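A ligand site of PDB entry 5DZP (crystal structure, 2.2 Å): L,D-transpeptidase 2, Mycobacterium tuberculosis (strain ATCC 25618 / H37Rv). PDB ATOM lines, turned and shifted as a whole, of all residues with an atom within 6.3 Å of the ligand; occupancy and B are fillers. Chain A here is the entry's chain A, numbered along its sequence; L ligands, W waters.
Water W4 bridges OG of Ser 293 (2.5 Å) and O4 of the ligand (3.0 Å).
Water W2 lies within hydrogen-bond range of N of Ala 250, OH of Tyr 254 and O3 of the ligand.
The side-chain sulfur of Cys 316 sits at hydrogen-bond distance from the backbone NH of Phe 296 (3.6 Å).
The side-chain hydroxyl (OG) of Ser 313 sits at hydrogen-bond distance from the backbone carbonyl oxygen (O) of Cys 316 (2.8 Å).
OG of Ser 291 is in hydrogen-bond range of N of Gly 294, at 3.3 Å.
The side-chain hydroxyl of Ser 293 is in hydrogen-bond range of the side-chain hydroxyl of Ser 291, at 2.6 Å.
N of Gly 315 is in hydrogen-bond range of OG of Ser 313 (2.9 Å).
The backbone NH of Val 295 lies within hydrogen-bond range of the side-chain hydroxyl of Ser 291, at 3.1 Å.
O of Ser 313 sits at hydrogen-bond distance from OG1 of Thr 247 (3.2 Å).
The backbone carbonyl oxygen of Thr 282 is in hydrogen-bond range of the backbone NH of Met 265, at 2.8 Å.
N of Cys 316 sits close to O5 of the ligand (2.9 Å).
C4 of the ligand is covalently linked to SG of Cys 316, at 1.7 Å.
O of Gly 294 is in hydrogen-bond range of O6 of the ligand (2.8 Å).
An oxygen (O5) of the ligand is in hydrogen-bond range of the backbone NH of Gly 315 (3.4 Å).
O6 of the ligand sits close to SD of Met 265, 3.8 Å away.
The backbone carbonyl oxygen (O) of His 314 lies close to a sulfur (S1) of the ligand (3.5 Å).
Ser 246 touches the ligand (O to C9, 3.98 Å).
Thr 247 touches the ligand.
O of Pro 248 touches O3 of the ligand, at 3.99 Å.
Asn 278 touches the ligand.
OH of Tyr 280 touches C15 of the ligand (3.1 Å).
Ser 293 touches the ligand (O to C1, 3.1 Å).
Val 295 touches the ligand.
Hydrophobic or aromatic side chains within 4 Å of the ligand: Met 265, Tyr 280, Val 295 and His 314.
Of the 25 residues printed, 12 come within 4 Å of the ligand.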
ATOM      1  N   SER A 246       7.413 -19.347 -27.087  1.00  0.00           N
ATOM      2  CA  SER A 246       6.116 -19.997 -27.257  1.00  0.00           C
ATOM      3  C   SER A 246       4.972 -19.218 -26.640  1.00  0.00           C
ATOM      4  O   SER A 246       3.796 -19.470 -26.966  1.00  0.00           O
ATOM      5  CB  SER A 246       6.146 -21.431 -26.713  1.00  0.00           C
ATOM      6  OG  SER A 246       6.329 -21.431 -25.311  1.00  0.00           O
ATOM      7  N   THR A 247       5.289 -18.305 -25.723  1.00  0.00           N
ATOM      8  CA  THR A 247       4.311 -17.368 -25.196  1.00  0.00           C
ATOM      9  C   THR A 247       4.939 -15.957 -25.246  1.00  0.00           C
ATOM     10  O   THR A 247       5.183 -15.332 -24.201  1.00  0.00           O
ATOM     11  CB  THR A 247       3.984 -17.721 -23.767  1.00  0.00           C
ATOM     12  OG1 THR A 247       5.227 -17.880 -23.077  1.00  0.00           O
ATOM     13  CG2 THR A 247       3.208 -19.012 -23.690  1.00  0.00           C
ATOM     14  N   PRO A 248       5.248 -15.451 -26.464  1.00  0.00           N
ATOM     15  CA  PRO A 248       5.989 -14.189 -26.579  1.00  0.00           C
ATOM     16  C   PRO A 248       5.225 -12.925 -26.053  1.00  0.00           C
ATOM     17  O   PRO A 248       4.018 -12.967 -25.817  1.00  0.00           O
ATOM     18  CB  PRO A 248       6.233 -14.083 -28.092  1.00  0.00           C
ATOM     19  CG  PRO A 248       5.061 -14.786 -28.715  1.00  0.00           C
ATOM     20  CD  PRO A 248       4.763 -15.922 -27.775  1.00  0.00           C
ATOM     21  N   THR A 249       5.952 -11.830 -25.837  1.00  0.00           N
ATOM     22  CA  THR A 249       5.317 -10.553 -25.520  1.00  0.00           C
ATOM     23  C   THR A 249       4.961  -9.940 -26.869  1.00  0.00           C
ATOM     24  O   THR A 249       5.808  -9.846 -27.782  1.00  0.00           O
ATOM     25  CB  THR A 249       6.269  -9.672 -24.690  1.00  0.00           C
ATOM     26  OG1 THR A 249       6.594 -10.351 -23.474  1.00  0.00           O
ATOM     27  CG2 THR A 249       5.655  -8.290 -24.374  1.00  0.00           C
ATOM     28  N   ALA A 250       3.697  -9.553 -27.020  1.00  0.00           N
ATOM     29  CA  ALA A 250       3.252  -8.834 -28.197  1.00  0.00           C
ATOM     30  C   ALA A 250       3.965  -7.464 -28.262  1.00  0.00           C
ATOM     31  O   ALA A 250       4.168  -6.797 -27.212  1.00  0.00           O
ATOM     32  CB  ALA A 250       1.732  -8.699 -28.195  1.00  0.00           C
ATOM     33  N   TYR A 254       1.643   0.086 -25.170  1.00  0.00           N
ATOM     34  CA  TYR A 254       0.753  -0.280 -24.091  1.00  0.00           C
ATOM     35  C   TYR A 254       0.560   0.958 -23.203  1.00  0.00           C
ATOM     36  O   TYR A 254       1.519   1.689 -22.937  1.00  0.00           O
ATOM     37  CB  TYR A 254       1.392  -1.345 -23.213  1.00  0.00           C
ATOM     38  CG  TYR A 254       1.651  -2.710 -23.802  1.00  0.00           C
ATOM     39  CD1 TYR A 254       2.579  -2.894 -24.827  1.00  0.00           C
ATOM     40  CD2 TYR A 254       1.032  -3.839 -23.250  1.00  0.00           C
ATOM     41  CE1 TYR A 254       2.842  -4.152 -25.369  1.00  0.00           C
ATOM     42  CE2 TYR A 254       1.305  -5.150 -23.750  1.00  0.00           C
ATOM     43  CZ  TYR A 254       2.197  -5.296 -24.811  1.00  0.00           C
ATOM     44  OH  TYR A 254       2.452  -6.556 -25.304  1.00  0.00           O
ATOM     45  N   MET A 265      -1.647 -13.203  -9.344  1.00  0.00           N
ATOM     46  CA  MET A 265      -1.895 -13.420 -10.746  1.00  0.00           C
ATOM     47  C   MET A 265      -2.557 -14.749 -10.952  1.00  0.00           C
ATOM     48  O   MET A 265      -1.896 -15.781 -10.805  1.00  0.00           O
ATOM     49  CB  MET A 265      -0.588 -13.576 -11.494  1.00  0.00           C
ATOM     50  CG  MET A 265       0.380 -12.476 -11.329  1.00  0.00           C
ATOM     51  SD  MET A 265      -0.264 -10.999 -12.049  1.00  0.00           S
ATOM     52  CE  MET A 265       1.343 -10.601 -12.783  1.00  0.00           C
ATOM     53  N   ASP A 266      -3.803 -14.700 -11.409  1.00  0.00           N
ATOM     54  CA  ASP A 266      -4.643 -15.859 -11.560  1.00  0.00           C
ATOM     55  C   ASP A 266      -4.979 -15.914 -13.039  1.00  0.00           C
ATOM     56  O   ASP A 266      -5.591 -14.974 -13.565  1.00  0.00           O
ATOM     57  CB  ASP A 266      -5.927 -15.653 -10.722  1.00  0.00           C
ATOM     58  CG  ASP A 266      -6.788 -16.921 -10.592  1.00  0.00           C
ATOM     59  OD1 ASP A 266      -6.736 -17.839 -11.451  1.00  0.00           O
ATOM     60  OD2 ASP A 266      -7.557 -16.988  -9.587  1.00  0.00           O
ATOM     61  N   TYR A 270      -7.991 -14.224 -16.862  1.00  0.00           N
ATOM     62  CA  TYR A 270      -7.790 -14.019 -18.312  1.00  0.00           C
ATOM     63  C   TYR A 270      -8.151 -15.245 -19.137  1.00  0.00           C
ATOM     64  O   TYR A 270      -7.566 -15.428 -20.188  1.00  0.00           O
ATOM     65  CB  TYR A 270      -6.358 -13.510 -18.634  1.00  0.00           C
ATOM     66  CG  TYR A 270      -5.894 -12.490 -17.640  1.00  0.00           C
ATOM     67  CD1 TYR A 270      -6.355 -11.157 -17.680  1.00  0.00           C
ATOM     68  CD2 TYR A 270      -5.050 -12.859 -16.602  1.00  0.00           C
ATOM     69  CE1 TYR A 270      -5.984 -10.205 -16.696  1.00  0.00           C
ATOM     70  CE2 TYR A 270      -4.645 -11.941 -15.633  1.00  0.00           C
ATOM     71  CZ  TYR A 270      -5.108 -10.614 -15.665  1.00  0.00           C
ATOM     72  OH  TYR A 270      -4.690  -9.750 -14.682  1.00  0.00           O
ATOM     73  N   VAL A 272      -7.799 -18.550 -18.923  1.00  0.00           N
ATOM     74  CA  VAL A 272      -6.961 -19.772 -18.929  1.00  0.00           C
ATOM     75  C   VAL A 272      -7.053 -20.552 -17.593  1.00  0.00           C
ATOM     76  O   VAL A 272      -6.725 -19.998 -16.545  1.00  0.00           O
ATOM     77  CB  VAL A 272      -5.467 -19.421 -19.206  1.00  0.00           C
ATOM     78  CG1 VAL A 272      -4.632 -20.686 -19.422  1.00  0.00           C
ATOM     79  CG2 VAL A 272      -5.321 -18.408 -20.359  1.00  0.00           C
ATOM     80  N   ASN A 278      -0.951 -23.919 -19.765  1.00  0.00           N
ATOM     81  CA  ASN A 278      -0.443 -22.533 -19.761  1.00  0.00           C
ATOM     82  C   ASN A 278      -0.857 -21.666 -18.560  1.00  0.00           C
ATOM     83  O   ASN A 278      -0.487 -20.500 -18.494  1.00  0.00           O
ATOM     84  CB  ASN A 278      -0.863 -21.823 -21.057  1.00  0.00           C
ATOM     85  CG  ASN A 278       0.223 -21.813 -22.119  1.00  0.00           C
ATOM     86  OD1 ASN A 278       1.413 -21.969 -21.850  1.00  0.00           O
ATOM     87  ND2 ASN A 278      -0.188 -21.613 -23.354  1.00  0.00           N
ATOM     88  N   TYR A 280      -1.591 -20.595 -14.333  1.00  0.00           N
ATOM     89  CA  TYR A 280      -0.704 -20.187 -13.227  1.00  0.00           C
ATOM     90  C   TYR A 280      -1.524 -19.507 -12.147  1.00  0.00           C
ATOM     91  O   TYR A 280      -2.585 -18.915 -12.403  1.00  0.00           O
ATOM     92  CB  TYR A 280       0.424 -19.225 -13.717  1.00  0.00           C
ATOM     93  CG  TYR A 280      -0.151 -18.111 -14.570  1.00  0.00           C
ATOM     94  CD1 TYR A 280      -0.776 -17.020 -13.982  1.00  0.00           C
ATOM     95  CD2 TYR A 280      -0.173 -18.205 -15.973  1.00  0.00           C
ATOM     96  CE1 TYR A 280      -1.375 -16.048 -14.745  1.00  0.00           C
ATOM     97  CE2 TYR A 280      -0.771 -17.214 -16.774  1.00  0.00           C
ATOM     98  CZ  TYR A 280      -1.366 -16.135 -16.131  1.00  0.00           C
ATOM     99  OH  TYR A 280      -1.966 -15.137 -16.832  1.00  0.00           O
ATOM    100  N   THR A 282       0.234 -17.254  -8.925  1.00  0.00           N
ATOM    101  CA  THR A 282       1.459 -16.817  -8.268  1.00  0.00           C
ATOM    102  C   THR A 282       1.218 -15.437  -7.701  1.00  0.00           C
ATOM    103  O   THR A 282       0.591 -14.584  -8.369  1.00  0.00           O
ATOM    104  CB  THR A 282       2.619 -16.661  -9.251  1.00  0.00           C
ATOM    105  OG1 THR A 282       2.188 -15.814 -10.333  1.00  0.00           O
ATOM    106  CG2 THR A 282       3.087 -18.014  -9.802  1.00  0.00           C
ATOM    107  N   SER A 291      -1.552  -4.356 -19.913  1.00  0.00           N
ATOM    108  CA  SER A 291      -2.677  -4.742 -20.785  1.00  0.00           C
ATOM    109  C   SER A 291      -3.833  -5.446 -20.017  1.00  0.00           C
ATOM    110  O   SER A 291      -3.629  -6.039 -18.952  1.00  0.00           O
ATOM    111  CB  SER A 291      -2.219  -5.604 -21.924  1.00  0.00           C
ATOM    112  OG  SER A 291      -2.066  -6.938 -21.440  1.00  0.00           O
ATOM    113  N   SER A 293      -5.246  -7.950 -21.292  1.00  0.00           N
ATOM    114  CA  SER A 293      -4.926  -9.374 -21.488  1.00  0.00           C
ATOM    115  C   SER A 293      -4.012  -9.939 -20.394  1.00  0.00           C
ATOM    116  O   SER A 293      -3.727 -11.118 -20.419  1.00  0.00           O
ATOM    117  CB  SER A 293      -4.280  -9.545 -22.855  1.00  0.00           C
ATOM    118  OG  SER A 293      -2.980  -9.000 -22.781  1.00  0.00           O
ATOM    119  N   GLY A 294      -3.551  -9.099 -19.453  1.00  0.00           N
ATOM    120  CA  GLY A 294      -2.765  -9.523 -18.280  1.00  0.00           C
ATOM    121  C   GLY A 294      -1.224  -9.367 -18.267  1.00  0.00           C
ATOM    122  O   GLY A 294      -0.568  -9.919 -17.397  1.00  0.00           O
ATOM    123  N   VAL A 295      -0.664  -8.640 -19.235  1.00  0.00           N
ATOM    124  CA  VAL A 295       0.738  -8.249 -19.234  1.00  0.00           C
ATOM    125  C   VAL A 295       1.027  -7.234 -18.137  1.00  0.00           C
ATOM    126  O   VAL A 295       0.362  -6.179 -18.065  1.00  0.00           O
ATOM    127  CB  VAL A 295       1.166  -7.654 -20.576  1.00  0.00           C
ATOM    128  CG1 VAL A 295       2.671  -7.277 -20.518  1.00  0.00           C
ATOM    129  CG2 VAL A 295       0.980  -8.679 -21.680  1.00  0.00           C
ATOM    130  N   PHE A 296       1.978  -7.573 -17.262  1.00  0.00           N
ATOM    131  CA  PHE A 296       2.446  -6.675 -16.190  1.00  0.00           C
ATOM    132  C   PHE A 296       3.951  -6.552 -16.285  1.00  0.00           C
ATOM    133  O   PHE A 296       4.615  -7.472 -16.786  1.00  0.00           O
ATOM    134  CB  PHE A 296       2.150  -7.224 -14.788  1.00  0.00           C
ATOM    135  CG  PHE A 296       0.717  -7.155 -14.361  1.00  0.00           C
ATOM    136  CD1 PHE A 296      -0.236  -8.099 -14.811  1.00  0.00           C
ATOM    137  CD2 PHE A 296       0.323  -6.224 -13.450  1.00  0.00           C
ATOM    138  CE1 PHE A 296      -1.553  -8.057 -14.375  1.00  0.00           C
ATOM    139  CE2 PHE A 296      -1.003  -6.170 -12.995  1.00  0.00           C
ATOM    140  CZ  PHE A 296      -1.942  -7.076 -13.462  1.00  0.00           C
ATOM    141  N   HIS A 298       6.657  -6.557 -13.408  1.00  0.00           N
ATOM    142  CA  HIS A 298       6.624  -6.965 -12.003  1.00  0.00           C
ATOM    143  C   HIS A 298       7.961  -7.508 -11.520  1.00  0.00           C
ATOM    144  O   HIS A 298       8.856  -7.800 -12.323  1.00  0.00           O
ATOM    145  CB  HIS A 298       5.481  -7.981 -11.739  1.00  0.00           C
ATOM    146  CG  HIS A 298       5.695  -9.314 -12.386  1.00  0.00           C
ATOM    147  ND1 HIS A 298       6.558 -10.257 -11.860  1.00  0.00           N
ATOM    148  CD2 HIS A 298       5.216  -9.849 -13.517  1.00  0.00           C
ATOM    149  CE1 HIS A 298       6.568 -11.321 -12.651  1.00  0.00           C
ATOM    150  NE2 HIS A 298       5.761 -11.094 -13.656  1.00  0.00           N
ATOM    151  N   SER A 313       9.393 -15.676 -19.561  1.00  0.00           N
ATOM    152  CA  SER A 313       8.064 -15.505 -18.918  1.00  0.00           C
ATOM    153  C   SER A 313       6.907 -16.029 -19.779  1.00  0.00           C
ATOM    154  O   SER A 313       7.107 -16.419 -20.932  1.00  0.00           O
ATOM    155  CB  SER A 313       7.809 -14.003 -18.579  1.00  0.00           C
ATOM    156  OG  SER A 313       7.455 -13.260 -19.755  1.00  0.00           O
ATOM    157  N   HIS A 314       5.694 -15.966 -19.218  1.00  0.00           N
ATOM    158  CA  HIS A 314       4.445 -16.097 -19.944  1.00  0.00           C
ATOM    159  C   HIS A 314       4.092 -14.898 -20.845  1.00  0.00           C
ATOM    160  O   HIS A 314       3.169 -14.985 -21.624  1.00  0.00           O
ATOM    161  CB  HIS A 314       3.293 -16.329 -18.967  1.00  0.00           C
ATOM    162  CG  HIS A 314       3.388 -17.621 -18.215  1.00  0.00           C
ATOM    163  ND1 HIS A 314       3.505 -17.685 -16.850  1.00  0.00           N
ATOM    164  CD2 HIS A 314       3.398 -18.899 -18.656  1.00  0.00           C
ATOM    165  CE1 HIS A 314       3.578 -18.950 -16.476  1.00  0.00           C
ATOM    166  NE2 HIS A 314       3.509 -19.712 -17.551  1.00  0.00           N
ATOM    167  N   GLY A 315       4.803 -13.788 -20.704  1.00  0.00           N
ATOM    168  CA  GLY A 315       4.509 -12.596 -21.519  1.00  0.00           C
ATOM    169  C   GLY A 315       4.790 -11.300 -20.803  1.00  0.00           C
ATOM    170  O   GLY A 315       5.020 -10.308 -21.429  1.00  0.00           O
ATOM    171  N   CYS A 316       4.737 -11.350 -19.466  1.00  0.00           N
ATOM    172  CA  CYS A 316       5.108 -10.284 -18.537  1.00  0.00           C
ATOM    173  C   CYS A 316       6.535  -9.805 -18.671  1.00  0.00           C
ATOM    174  O   CYS A 316       7.408 -10.555 -19.100  1.00  0.00           O
ATOM    175  CB  CYS A 316       4.904 -10.755 -17.103  1.00  0.00           C
ATOM    176  SG  CYS A 316       3.146 -10.886 -16.737  1.00  0.00           S
ATOM    177  N   LEU A 317       6.768  -8.555 -18.292  1.00  0.00           N
ATOM    178  CA  LEU A 317       8.096  -7.972 -18.326  1.00  0.00           C
ATOM    179  C   LEU A 317       8.634  -8.173 -16.948  1.00  0.00           C
ATOM    180  O   LEU A 317       8.340  -7.427 -16.013  1.00  0.00           O
ATOM    181  CB  LEU A 317       8.055  -6.504 -18.724  1.00  0.00           C
ATOM    182  CG  LEU A 317       8.017  -6.177 -20.236  1.00  0.00           C
ATOM    183  CD1 LEU A 317       6.943  -6.943 -21.006  1.00  0.00           C
ATOM    184  CD2 LEU A 317       7.847  -4.669 -20.532  1.00  0.00           C
ATOM    185  N   ASN A 318       9.424  -9.246 -16.824  1.00  0.00           N
ATOM    186  CA  ASN A 318      10.082  -9.545 -15.601  1.00  0.00           C
ATOM    187  C   ASN A 318      11.280  -8.617 -15.485  1.00  0.00           C
ATOM    188  O   ASN A 318      11.973  -8.427 -16.447  1.00  0.00           O
ATOM    189  CB  ASN A 318      10.604 -10.971 -15.666  1.00  0.00           C
ATOM    190  CG  ASN A 318       9.535 -12.017 -15.397  1.00  0.00           C
ATOM    191  OD1 ASN A 318       8.323 -11.740 -15.402  1.00  0.00           O
ATOM    192  ND2 ASN A 318       9.998 -13.241 -15.146  1.00  0.00           N
HETATM  193  C1  LIG L   1      -1.688 -13.223 -19.422  1.00  0.00           C
HETATM  194  C2  LIG L   1       0.919 -13.267 -18.820  1.00  0.00           C
HETATM  195  C3  LIG L   1       1.286 -12.620 -17.427  1.00  0.00           C
HETATM  196  N1  LIG L   1       1.267 -12.446 -20.023  1.00  0.00           N
HETATM  197  C4  LIG L   1       2.816 -12.420 -17.248  1.00  0.00           C
HETATM  198  C5  LIG L   1       0.531 -13.102 -16.134  1.00  0.00           C
HETATM  199  C6  LIG L   1       1.393 -13.623 -14.957  1.00  0.00           C
HETATM  200  S1  LIG L   1      -0.165 -15.925 -21.787  1.00  0.00           S
HETATM  201  C7  LIG L   1      -1.583 -16.172 -24.259  1.00  0.00           C
HETATM  202  O1  LIG L   1      -2.644 -16.352 -24.858  1.00  0.00           O
HETATM  203  O2  LIG L   1      -0.287 -16.485 -24.749  1.00  0.00           O
HETATM  204  C8  LIG L   1      -0.073 -17.284 -25.959  1.00  0.00           C
HETATM  205  O3  LIG L   1       1.509 -11.889 -22.907  1.00  0.00           O
HETATM  206  C9  LIG L   1       0.107 -18.779 -25.635  1.00  0.00           C
HETATM  207  O4  LIG L   1      -0.729 -12.531 -22.751  1.00  0.00           O
HETATM  208  C10 LIG L   1      -0.733 -19.767 -26.440  1.00  0.00           C
HETATM  209  O5  LIG L   1       3.655 -13.284 -17.541  1.00  0.00           O
HETATM  210  C11 LIG L   1      -1.629 -15.530 -22.857  1.00  0.00           C
HETATM  211  O6  LIG L   1      -0.432 -12.078 -15.679  1.00  0.00           O
HETATM  212  C12 LIG L   1       0.281 -14.557 -20.544  1.00  0.00           C
HETATM  213  C13 LIG L   1       0.813 -13.180 -21.010  1.00  0.00           C
HETATM  214  C14 LIG L   1       0.501 -12.491 -22.361  1.00  0.00           C
HETATM  215  C15 LIG L   1      -0.397 -14.047 -19.266  1.00  0.00           C
HETATM  216  O   HOH W   1      -0.673 -13.633 -26.582  1.00  0.00           O
HETATM  217  O   HOH W   2       1.647  -9.419 -24.925  1.00  0.00           O
HETATM  218  O   HOH W   3       6.106 -14.960 -15.889  1.00  0.00           O
HETATM  219  O   HOH W   4      -1.450 -10.116 -24.342  1.00  0.00           O
HETATM  220  O   HOH W   5       2.318 -14.151 -24.398  1.00  0.00           O
